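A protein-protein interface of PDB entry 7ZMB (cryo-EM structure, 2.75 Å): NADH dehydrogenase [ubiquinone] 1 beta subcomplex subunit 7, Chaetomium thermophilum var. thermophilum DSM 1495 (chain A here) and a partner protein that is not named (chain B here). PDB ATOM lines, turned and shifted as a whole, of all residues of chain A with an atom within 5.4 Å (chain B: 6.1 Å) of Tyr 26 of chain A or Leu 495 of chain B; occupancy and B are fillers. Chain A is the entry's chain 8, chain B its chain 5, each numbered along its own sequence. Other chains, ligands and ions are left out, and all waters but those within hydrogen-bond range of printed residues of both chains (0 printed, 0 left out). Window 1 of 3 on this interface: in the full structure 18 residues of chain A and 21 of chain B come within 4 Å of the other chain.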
ATOM      1  N   VAL A  22     -28.350 -21.052 -10.424  1.00  0.00           N
ATOM      2  CA  VAL A  22     -27.053 -20.920  -9.769  1.00  0.00           C
ATOM      3  C   VAL A  22     -27.285 -20.635  -8.288  1.00  0.00           C
ATOM      4  O   VAL A  22     -28.355 -20.132  -7.920  1.00  0.00           O
ATOM      5  CB  VAL A  22     -26.208 -19.824 -10.436  1.00  0.00           C
ATOM      6  CG1 VAL A  22     -26.075 -20.101 -11.922  1.00  0.00           C
ATOM      7  CG2 VAL A  22     -26.819 -18.464 -10.196  1.00  0.00           C
ATOM      8  N   PRO A  23     -26.331 -20.944  -7.409  1.00  0.00           N
ATOM      9  CA  PRO A  23     -26.567 -20.776  -5.970  1.00  0.00           C
ATOM     10  C   PRO A  23     -26.792 -19.320  -5.586  1.00  0.00           C
ATOM     11  O   PRO A  23     -26.389 -18.390  -6.288  1.00  0.00           O
ATOM     12  CB  PRO A  23     -25.284 -21.323  -5.333  1.00  0.00           C
ATOM     13  CG  PRO A  23     -24.712 -22.235  -6.361  1.00  0.00           C
ATOM     14  CD  PRO A  23     -25.049 -21.616  -7.679  1.00  0.00           C
ATOM     15  N   LEU A  24     -27.459 -19.137  -4.442  1.00  0.00           N
ATOM     16  CA  LEU A  24     -27.796 -17.793  -3.983  1.00  0.00           C
ATOM     17  C   LEU A  24     -26.547 -16.966  -3.715  1.00  0.00           C
ATOM     18  O   LEU A  24     -26.493 -15.779  -4.059  1.00  0.00           O
ATOM     19  CB  LEU A  24     -28.654 -17.856  -2.717  1.00  0.00           C
ATOM     20  CG  LEU A  24     -30.164 -18.080  -2.827  1.00  0.00           C
ATOM     21  CD1 LEU A  24     -30.821 -16.977  -3.647  1.00  0.00           C
ATOM     22  CD2 LEU A  24     -30.497 -19.449  -3.372  1.00  0.00           C
ATOM     23  N   ALA A  25     -25.532 -17.570  -3.096  1.00  0.00           N
ATOM     24  CA  ALA A  25     -24.326 -16.834  -2.742  1.00  0.00           C
ATOM     25  C   ALA A  25     -23.528 -16.384  -3.956  1.00  0.00           C
ATOM     26  O   ALA A  25     -22.606 -15.575  -3.803  1.00  0.00           O
ATOM     27  CB  ALA A  25     -23.442 -17.684  -1.831  1.00  0.00           C
ATOM     28  N   TYR A  26     -23.850 -16.882  -5.147  1.00  0.00           N
ATOM     29  CA  TYR A  26     -23.131 -16.538  -6.365  1.00  0.00           C
ATOM     30  C   TYR A  26     -24.040 -15.856  -7.381  1.00  0.00           C
ATOM     31  O   TYR A  26     -23.776 -15.892  -8.584  1.00  0.00           O
ATOM     32  CB  TYR A  26     -22.481 -17.782  -6.969  1.00  0.00           C
ATOM     33  CG  TYR A  26     -21.597 -18.524  -5.994  1.00  0.00           C
ATOM     34  CD1 TYR A  26     -20.763 -17.838  -5.125  1.00  0.00           C
ATOM     35  CD2 TYR A  26     -21.607 -19.909  -5.935  1.00  0.00           C
ATOM     36  CE1 TYR A  26     -19.957 -18.508  -4.229  1.00  0.00           C
ATOM     37  CE2 TYR A  26     -20.804 -20.589  -5.041  1.00  0.00           C
ATOM     38  CZ  TYR A  26     -19.982 -19.884  -4.192  1.00  0.00           C
ATOM     39  OH  TYR A  26     -19.180 -20.557  -3.301  1.00  0.00           O
ATOM     40  N   ARG A  27     -25.116 -15.229  -6.910  1.00  0.00           N
ATOM     41  CA  ARG A  27     -25.990 -14.437  -7.767  1.00  0.00           C
ATOM     42  C   ARG A  27     -25.406 -13.076  -8.115  1.00  0.00           C
ATOM     43  O   ARG A  27     -26.122 -12.242  -8.678  1.00  0.00           O
ATOM     44  CB  ARG A  27     -27.357 -14.240  -7.105  1.00  0.00           C
ATOM     45  CG  ARG A  27     -28.133 -15.510  -6.820  1.00  0.00           C
ATOM     46  CD  ARG A  27     -28.576 -16.149  -8.115  1.00  0.00           C
ATOM     47  NE  ARG A  27     -29.325 -17.383  -7.917  1.00  0.00           N
ATOM     48  CZ  ARG A  27     -30.647 -17.429  -7.783  1.00  0.00           C
ATOM     49  NH1 ARG A  27     -31.355 -16.310  -7.826  1.00  0.00           N
ATOM     50  NH2 ARG A  27     -31.261 -18.589  -7.609  1.00  0.00           N
ATOM     51  N   ASP A  28     -24.137 -12.831  -7.799  1.00  0.00           N
ATOM     52  CA  ASP A  28     -23.545 -11.524  -8.022  1.00  0.00           C
ATOM     53  C   ASP A  28     -23.446 -11.220  -9.516  1.00  0.00           C
ATOM     54  O   ASP A  28     -23.656 -12.080 -10.376  1.00  0.00           O
ATOM     55  CB  ASP A  28     -22.165 -11.442  -7.369  1.00  0.00           C
ATOM     56  CG  ASP A  28     -21.200 -12.486  -7.900  1.00  0.00           C
ATOM     57  OD1 ASP A  28     -21.617 -13.336  -8.714  1.00  0.00           O
ATOM     58  OD2 ASP A  28     -20.016 -12.453  -7.503  1.00  0.00           O
ATOM     59  N   ALA A  31     -21.210 -13.363 -12.067  1.00  0.00           N
ATOM     60  CA  ALA A  31     -21.553 -14.744 -12.378  1.00  0.00           C
ATOM     61  C   ALA A  31     -21.809 -14.984 -13.861  1.00  0.00           C
ATOM     62  O   ALA A  31     -22.225 -16.088 -14.224  1.00  0.00           O
ATOM     63  CB  ALA A  31     -22.783 -15.170 -11.575  1.00  0.00           C
ATOM     64  N   LEU A  34     -19.961 -17.722 -14.799  1.00  0.00           N
ATOM     65  CA  LEU A  34     -20.269 -18.923 -14.033  1.00  0.00           C
ATOM     66  C   LEU A  34     -21.245 -19.831 -14.770  1.00  0.00           C
ATOM     67  O   LEU A  34     -21.162 -21.057 -14.636  1.00  0.00           O
ATOM     68  CB  LEU A  34     -20.820 -18.534 -12.657  1.00  0.00           C
ATOM     69  CG  LEU A  34     -21.058 -19.607 -11.590  1.00  0.00           C
ATOM     70  CD1 LEU A  34     -20.951 -18.988 -10.208  1.00  0.00           C
ATOM     71  CD2 LEU A  34     -22.416 -20.260 -11.744  1.00  0.00           C
ATOM     72  N   ARG A  41     -19.068 -28.805 -16.068  1.00  0.00           N
ATOM     73  CA  ARG A  41     -19.183 -29.812 -15.021  1.00  0.00           C
ATOM     74  C   ARG A  41     -20.351 -30.742 -15.309  1.00  0.00           C
ATOM     75  O   ARG A  41     -20.246 -31.964 -15.162  1.00  0.00           O
ATOM     76  CB  ARG A  41     -19.339 -29.134 -13.661  1.00  0.00           C
ATOM     77  CG  ARG A  41     -18.119 -28.334 -13.232  1.00  0.00           C
ATOM     78  CD  ARG A  41     -18.460 -27.347 -12.131  1.00  0.00           C
ATOM     79  NE  ARG A  41     -17.276 -26.649 -11.639  1.00  0.00           N
ATOM     80  CZ  ARG A  41     -17.316 -25.535 -10.916  1.00  0.00           C
ATOM     81  NH1 ARG A  41     -16.192 -24.966 -10.507  1.00  0.00           N
ATOM     82  NH2 ARG A  41     -18.483 -24.990 -10.605  1.00  0.00           N
ATOM     83  N   TYR A  58     -13.343 -18.136 -14.937  1.00  0.00           N
ATOM     84  CA  TYR A  58     -14.255 -17.640 -13.912  1.00  0.00           C
ATOM     85  C   TYR A  58     -13.492 -16.979 -12.773  1.00  0.00           C
ATOM     86  O   TYR A  58     -13.919 -15.940 -12.256  1.00  0.00           O
ATOM     87  CB  TYR A  58     -15.136 -18.772 -13.386  1.00  0.00           C
ATOM     88  CG  TYR A  58     -15.954 -18.383 -12.175  1.00  0.00           C
ATOM     89  CD1 TYR A  58     -17.198 -17.792 -12.318  1.00  0.00           C
ATOM     90  CD2 TYR A  58     -15.489 -18.624 -10.889  1.00  0.00           C
ATOM     91  CE1 TYR A  58     -17.947 -17.434 -11.219  1.00  0.00           C
ATOM     92  CE2 TYR A  58     -16.234 -18.272  -9.786  1.00  0.00           C
ATOM     93  CZ  TYR A  58     -17.463 -17.679  -9.955  1.00  0.00           C
ATOM     94  OH  TYR A  58     -18.212 -17.327  -8.859  1.00  0.00           O
ATOM     95  N   GLU A  59     -12.366 -17.565 -12.364  1.00  0.00           N
ATOM     96  CA  GLU A  59     -11.599 -16.995 -11.265  1.00  0.00           C
ATOM     97  C   GLU A  59     -10.964 -15.658 -11.631  1.00  0.00           C
ATOM     98  O   GLU A  59     -10.567 -14.914 -10.729  1.00  0.00           O
ATOM     99  CB  GLU A  59     -10.534 -17.986 -10.798  1.00  0.00           C
ATOM    100  CG  GLU A  59     -11.120 -19.233 -10.148  1.00  0.00           C
ATOM    101  CD  GLU A  59     -10.061 -20.220  -9.703  1.00  0.00           C
ATOM    102  OE1 GLU A  59      -8.871 -19.999 -10.011  1.00  0.00           O
ATOM    103  OE2 GLU A  59     -10.418 -21.219  -9.043  1.00  0.00           O
ATOM    104  N   GLN A  62     -13.671 -13.032 -10.371  1.00  0.00           N
ATOM    105  CA  GLN A  62     -13.685 -13.032  -8.912  1.00  0.00           C
ATOM    106  C   GLN A  62     -12.414 -12.404  -8.353  1.00  0.00           C
ATOM    107  O   GLN A  62     -12.465 -11.588  -7.426  1.00  0.00           O
ATOM    108  CB  GLN A  62     -13.856 -14.458  -8.391  1.00  0.00           C
ATOM    109  CG  GLN A  62     -15.225 -15.061  -8.656  1.00  0.00           C
ATOM    110  CD  GLN A  62     -16.324 -14.390  -7.859  1.00  0.00           C
ATOM    111  OE1 GLN A  62     -16.406 -14.546  -6.641  1.00  0.00           O
ATOM    112  NE2 GLN A  62     -17.179 -13.641  -8.543  1.00  0.00           N
ATOM    113  N   ASN B 323     -21.358 -27.765   2.447  1.00  0.00           N
ATOM    114  CA  ASN B 323     -20.684 -28.491   1.378  1.00  0.00           C
ATOM    115  C   ASN B 323     -19.313 -28.988   1.814  1.00  0.00           C
ATOM    116  O   ASN B 323     -18.928 -30.115   1.483  1.00  0.00           O
ATOM    117  CB  ASN B 323     -20.593 -27.611   0.132  1.00  0.00           C
ATOM    118  CG  ASN B 323     -20.009 -26.251   0.423  1.00  0.00           C
ATOM    119  OD1 ASN B 323     -19.652 -25.955   1.558  1.00  0.00           O
ATOM    120  ND2 ASN B 323     -19.905 -25.415  -0.602  1.00  0.00           N
ATOM    121  N   ASP B 490     -13.982 -30.917  -6.937  1.00  0.00           N
ATOM    122  CA  ASP B 490     -14.903 -30.006  -7.602  1.00  0.00           C
ATOM    123  C   ASP B 490     -16.345 -30.452  -7.396  1.00  0.00           C
ATOM    124  O   ASP B 490     -17.259 -29.622  -7.414  1.00  0.00           O
ATOM    125  CB  ASP B 490     -14.562 -29.926  -9.093  1.00  0.00           C
ATOM    126  CG  ASP B 490     -15.329 -28.834  -9.828  1.00  0.00           C
ATOM    127  OD1 ASP B 490     -16.157 -28.134  -9.213  1.00  0.00           O
ATOM    128  OD2 ASP B 490     -15.109 -28.680 -11.046  1.00  0.00           O
ATOM    129  N   ILE B 493     -16.570 -29.401  -3.147  1.00  0.00           N
ATOM    130  CA  ILE B 493     -16.001 -28.110  -2.781  1.00  0.00           C
ATOM    131  C   ILE B 493     -16.120 -27.150  -3.955  1.00  0.00           C
ATOM    132  O   ILE B 493     -16.863 -26.165  -3.888  1.00  0.00           O
ATOM    133  CB  ILE B 493     -14.530 -28.249  -2.345  1.00  0.00           C
ATOM    134  CG1 ILE B 493     -14.407 -29.230  -1.179  1.00  0.00           C
ATOM    135  CG2 ILE B 493     -13.958 -26.894  -1.971  1.00  0.00           C
ATOM    136  CD1 ILE B 493     -14.995 -28.720   0.106  1.00  0.00           C
ATOM    137  N   GLY B 494     -15.414 -27.452  -5.045  1.00  0.00           N
ATOM    138  CA  GLY B 494     -15.355 -26.578  -6.203  1.00  0.00           C
ATOM    139  C   GLY B 494     -15.126 -25.129  -5.834  1.00  0.00           C
ATOM    140  O   GLY B 494     -14.472 -24.837  -4.829  1.00  0.00           O
ATOM    141  N   LEU B 495     -15.639 -24.214  -6.635  1.00  0.00           N
ATOM    142  CA  LEU B 495     -15.735 -22.828  -6.196  1.00  0.00           C
ATOM    143  C   LEU B 495     -17.123 -22.256  -6.426  1.00  0.00           C
ATOM    144  O   LEU B 495     -17.620 -21.502  -5.586  1.00  0.00           O
ATOM    145  CB  LEU B 495     -14.681 -21.964  -6.908  1.00  0.00           C
ATOM    146  CG  LEU B 495     -14.343 -20.615  -6.265  1.00  0.00           C
ATOM    147  CD1 LEU B 495     -12.903 -20.235  -6.571  1.00  0.00           C
ATOM    148  CD2 LEU B 495     -15.283 -19.511  -6.713  1.00  0.00           C
ATOM    149  N   GLY B 496     -17.760 -22.600  -7.539  1.00  0.00           N
ATOM    150  CA  GLY B 496     -19.119 -22.186  -7.816  1.00  0.00           C
ATOM    151  C   GLY B 496     -19.955 -23.380  -8.219  1.00  0.00           C
ATOM    152  O   GLY B 496     -20.818 -23.282  -9.096  1.00  0.00           O
ATOM    153  N   SER B 497     -19.684 -24.519  -7.586  1.00  0.00           N
ATOM    154  CA  SER B 497     -20.331 -25.767  -7.961  1.00  0.00           C
ATOM    155  C   SER B 497     -21.843 -25.661  -7.824  1.00  0.00           C
ATOM    156  O   SER B 497     -22.360 -25.111  -6.846  1.00  0.00           O
ATOM    157  CB  SER B 497     -19.810 -26.912  -7.095  1.00  0.00           C
ATOM    158  OG  SER B 497     -20.378 -26.861  -5.799  1.00  0.00           O
ATOM    159  N   ILE B 507     -27.388 -22.343   1.783  1.00  0.00           N
ATOM    160  CA  ILE B 507     -26.381 -21.428   2.305  1.00  0.00           C
ATOM    161  C   ILE B 507     -26.848 -20.006   2.037  1.00  0.00           C
ATOM    162  O   ILE B 507     -27.404 -19.719   0.972  1.00  0.00           O
ATOM    163  CB  ILE B 507     -24.994 -21.686   1.682  1.00  0.00           C
ATOM    164  CG1 ILE B 507     -25.028 -21.474   0.168  1.00  0.00           C
ATOM    165  CG2 ILE B 507     -24.513 -23.086   2.014  1.00  0.00           C
ATOM    166  CD1 ILE B 507     -23.661 -21.481  -0.480  1.00  0.00           C
ATOM    167  N   PRO B 509     -26.213 -15.949   1.401  1.00  0.00           N
ATOM    168  CA  PRO B 509     -25.110 -15.081   0.957  1.00  0.00           C
ATOM    169  C   PRO B 509     -24.548 -14.178   2.042  1.00  0.00           C
ATOM    170  O   PRO B 509     -23.409 -13.717   1.904  1.00  0.00           O
ATOM    171  CB  PRO B 509     -25.743 -14.262  -0.177  1.00  0.00           C
ATOM    172  CG  PRO B 509     -27.221 -14.385   0.032  1.00  0.00           C
ATOM    173  CD  PRO B 509     -27.425 -15.750   0.591  1.00  0.00           C
ATOM    174  N   GLU B 512     -21.223 -15.773   3.332  1.00  0.00           N
ATOM    175  CA  GLU B 512     -20.401 -16.521   2.392  1.00  0.00           C
ATOM    176  C   GLU B 512     -18.929 -16.283   2.702  1.00  0.00           C
ATOM    177  O   GLU B 512     -18.506 -15.142   2.905  1.00  0.00           O
ATOM    178  CB  GLU B 512     -20.719 -16.106   0.957  1.00  0.00           C
ATOM    179  CG  GLU B 512     -19.922 -16.849  -0.102  1.00  0.00           C
ATOM    180  CD  GLU B 512     -18.604 -16.172  -0.419  1.00  0.00           C
ATOM    181  OE1 GLU B 512     -18.480 -14.960  -0.151  1.00  0.00           O
ATOM    182  OE2 GLU B 512     -17.692 -16.852  -0.932  1.00  0.00           O
ATOM    183  N   MET B 514     -16.591 -18.568   1.013  1.00  0.00           N
ATOM    184  CA  MET B 514     -15.909 -19.409   0.033  1.00  0.00           C
ATOM    185  C   MET B 514     -14.835 -18.632  -0.720  1.00  0.00           C
ATOM    186  O   MET B 514     -13.718 -19.128  -0.907  1.00  0.00           O
ATOM    187  CB  MET B 514     -16.924 -20.001  -0.942  1.00  0.00           C
ATOM    188  CG  MET B 514     -16.335 -21.012  -1.902  1.00  0.00           C
ATOM    189  SD  MET B 514     -15.757 -22.491  -1.055  1.00  0.00           S
ATOM    190  CE  MET B 514     -14.549 -23.082  -2.233  1.00  0.00           C
ATOM    191  N   ILE B 515     -15.153 -17.414  -1.162  1.00  0.00           N
ATOM    192  CA  ILE B 515     -14.174 -16.618  -1.897  1.00  0.00           C
ATOM    193  C   ILE B 515     -13.047 -16.163  -0.977  1.00  0.00           C
ATOM    194  O   ILE B 515     -11.880 -16.115  -1.384  1.00  0.00           O
ATOM    195  CB  ILE B 515     -14.861 -15.433  -2.598  1.00  0.00           C
ATOM    196  CG1 ILE B 515     -15.509 -14.497  -1.577  1.00  0.00           C
ATOM    197  CG2 ILE B 515     -15.890 -15.926  -3.600  1.00  0.00           C
ATOM    198  CD1 ILE B 515     -15.994 -13.207  -2.171  1.00  0.00           C
ATOM    199  N   GLU B 518     -10.162 -18.817  -0.239  1.00  0.00           N
ATOM    200  CA  GLU B 518      -9.119 -19.062  -1.225  1.00  0.00           C
ATOM    201  C   GLU B 518      -8.224 -17.856  -1.474  1.00  0.00           C
ATOM    202  O   GLU B 518      -7.072 -18.038  -1.887  1.00  0.00           O
ATOM    203  CB  GLU B 518      -9.750 -19.504  -2.553  1.00  0.00           C
ATOM    204  CG  GLU B 518      -8.763 -20.010  -3.593  1.00  0.00           C
ATOM    205  CD  GLU B 518      -9.361 -21.074  -4.494  1.00  0.00           C
ATOM    206  OE1 GLU B 518     -10.256 -21.811  -4.032  1.00  0.00           O
ATOM    207  OE2 GLU B 518      -8.937 -21.171  -5.665  1.00  0.00           O
ATOM    208  N   PHE B 519      -8.707 -16.640  -1.225  1.00  0.00           N
ATOM    209  CA  PHE B 519      -8.010 -15.428  -1.637  1.00  0.00           C
ATOM    210  C   PHE B 519      -7.472 -14.624  -0.460  1.00  0.00           C
ATOM    211  O   PHE B 519      -6.271 -14.350  -0.395  1.00  0.00           O
ATOM    212  CB  PHE B 519      -8.947 -14.557  -2.486  1.00  0.00           C
ATOM    213  CG  PHE B 519      -9.165 -15.072  -3.881  1.00  0.00           C
ATOM    214  CD1 PHE B 519      -8.641 -16.289  -4.283  1.00  0.00           C
ATOM    215  CD2 PHE B 519      -9.910 -14.342  -4.789  1.00  0.00           C
ATOM    216  CE1 PHE B 519      -8.845 -16.760  -5.561  1.00  0.00           C
ATOM    217  CE2 PHE B 519     -10.120 -14.809  -6.069  1.00  0.00           C
ATOM    218  CZ  PHE B 519      -9.586 -16.019  -6.455  1.00  0.00           C
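Among the printed residues, pairs that only touch across the chains: Tyr 26 of chain A with Met 514 of chain B, Gln 62 of chain A with Ile 515 of chain B, Tyr 58 of chain A with Leu 495 of chain B, Tyr 26 of chain A with Gly 496 of chain B, Glu 59 of chain A with Leu 495 of chain B, Glu 59 of chain A with Glu 518 of chain B, Pro 23 of chain A with Ser 497 of chain B, Ala 25 of chain A with Pro 509 of chain B and Arg 41 of chain A with Leu 495 of chain B.
The side-chain carboxylate of Glu 512 of chain B sits at hydrogen-bond distance from the backbone NH of Met 514 of chain B (2.8 Å). The backbone NH of Ile 515 of chain B is in hydrogen-bond range of the side-chain carboxylate of Glu 512 of chain B (2.6 Å). The side-chain amide nitrogen (NE2) of Gln 62 of chain A sits at hydrogen-bond distance from the side-chain carboxylate (OD2) of Asp 28 of chain A (3.2 Å).
Tyr 26 of chain A touches just these residues of chain B: Leu 495 (2.9 Å), Gly 496 (3.6 Å) and Met 514 (3.2 Å). Of the printed residues of chain A, Leu 495 of chain B touches Tyr 26, Arg 41, Tyr 58 and Glu 59. Printed residues of chain B within 4 Å of Arg 41 of chain A: Asp 490, Leu 495, Gly 496 and Ser 497. Printed residues of chain B within 4 Å of Ala 25 of chain A: Pro 509. Of the printed residues of chain B, Glu 59 of chain A touches Leu 495 and Glu 518. Printed residues of chain A within 4 Å of Met 514 of chain B: Tyr 26. Printed residues of chain B within 4 Å of Tyr 58 of chain A: Leu 495. The nearest residue of chain B that does not touch Tyr 26 of chain A is Glu 512 of chain B (4.3 Å). The nearest printed residue of chain A that does not touch Leu 495 of chain B is Gln 62 of chain A (4.9 Å).
Hydrophobic or aromatic side chains of chain B within 4 Å of the printed part of chain A: Leu 495, Pro 509, Met 514 and Ile 515. Of the 13 printed residues of chain A, 7 touch a printed residue of chain B.
The side-chain carboxylate (OD2) of Asp 490 of chain B is in salt-bridge range of the guanidinium group (NE) of Arg 41 of chain A, 3.0 Å away. O of Leu 495 of chain B lies within hydrogen-bond range of OH of Tyr 26 of chain A (2.9 Å). The backbone carbonyl oxygen of Gly 496 of chain B sits close to the guanidinium group of Arg 41 of chain A (3.3 Å). The guanidinium group (NH2) of Arg 41 of chain A lies close to the backbone NH (N) of Ser 497 of chain B.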
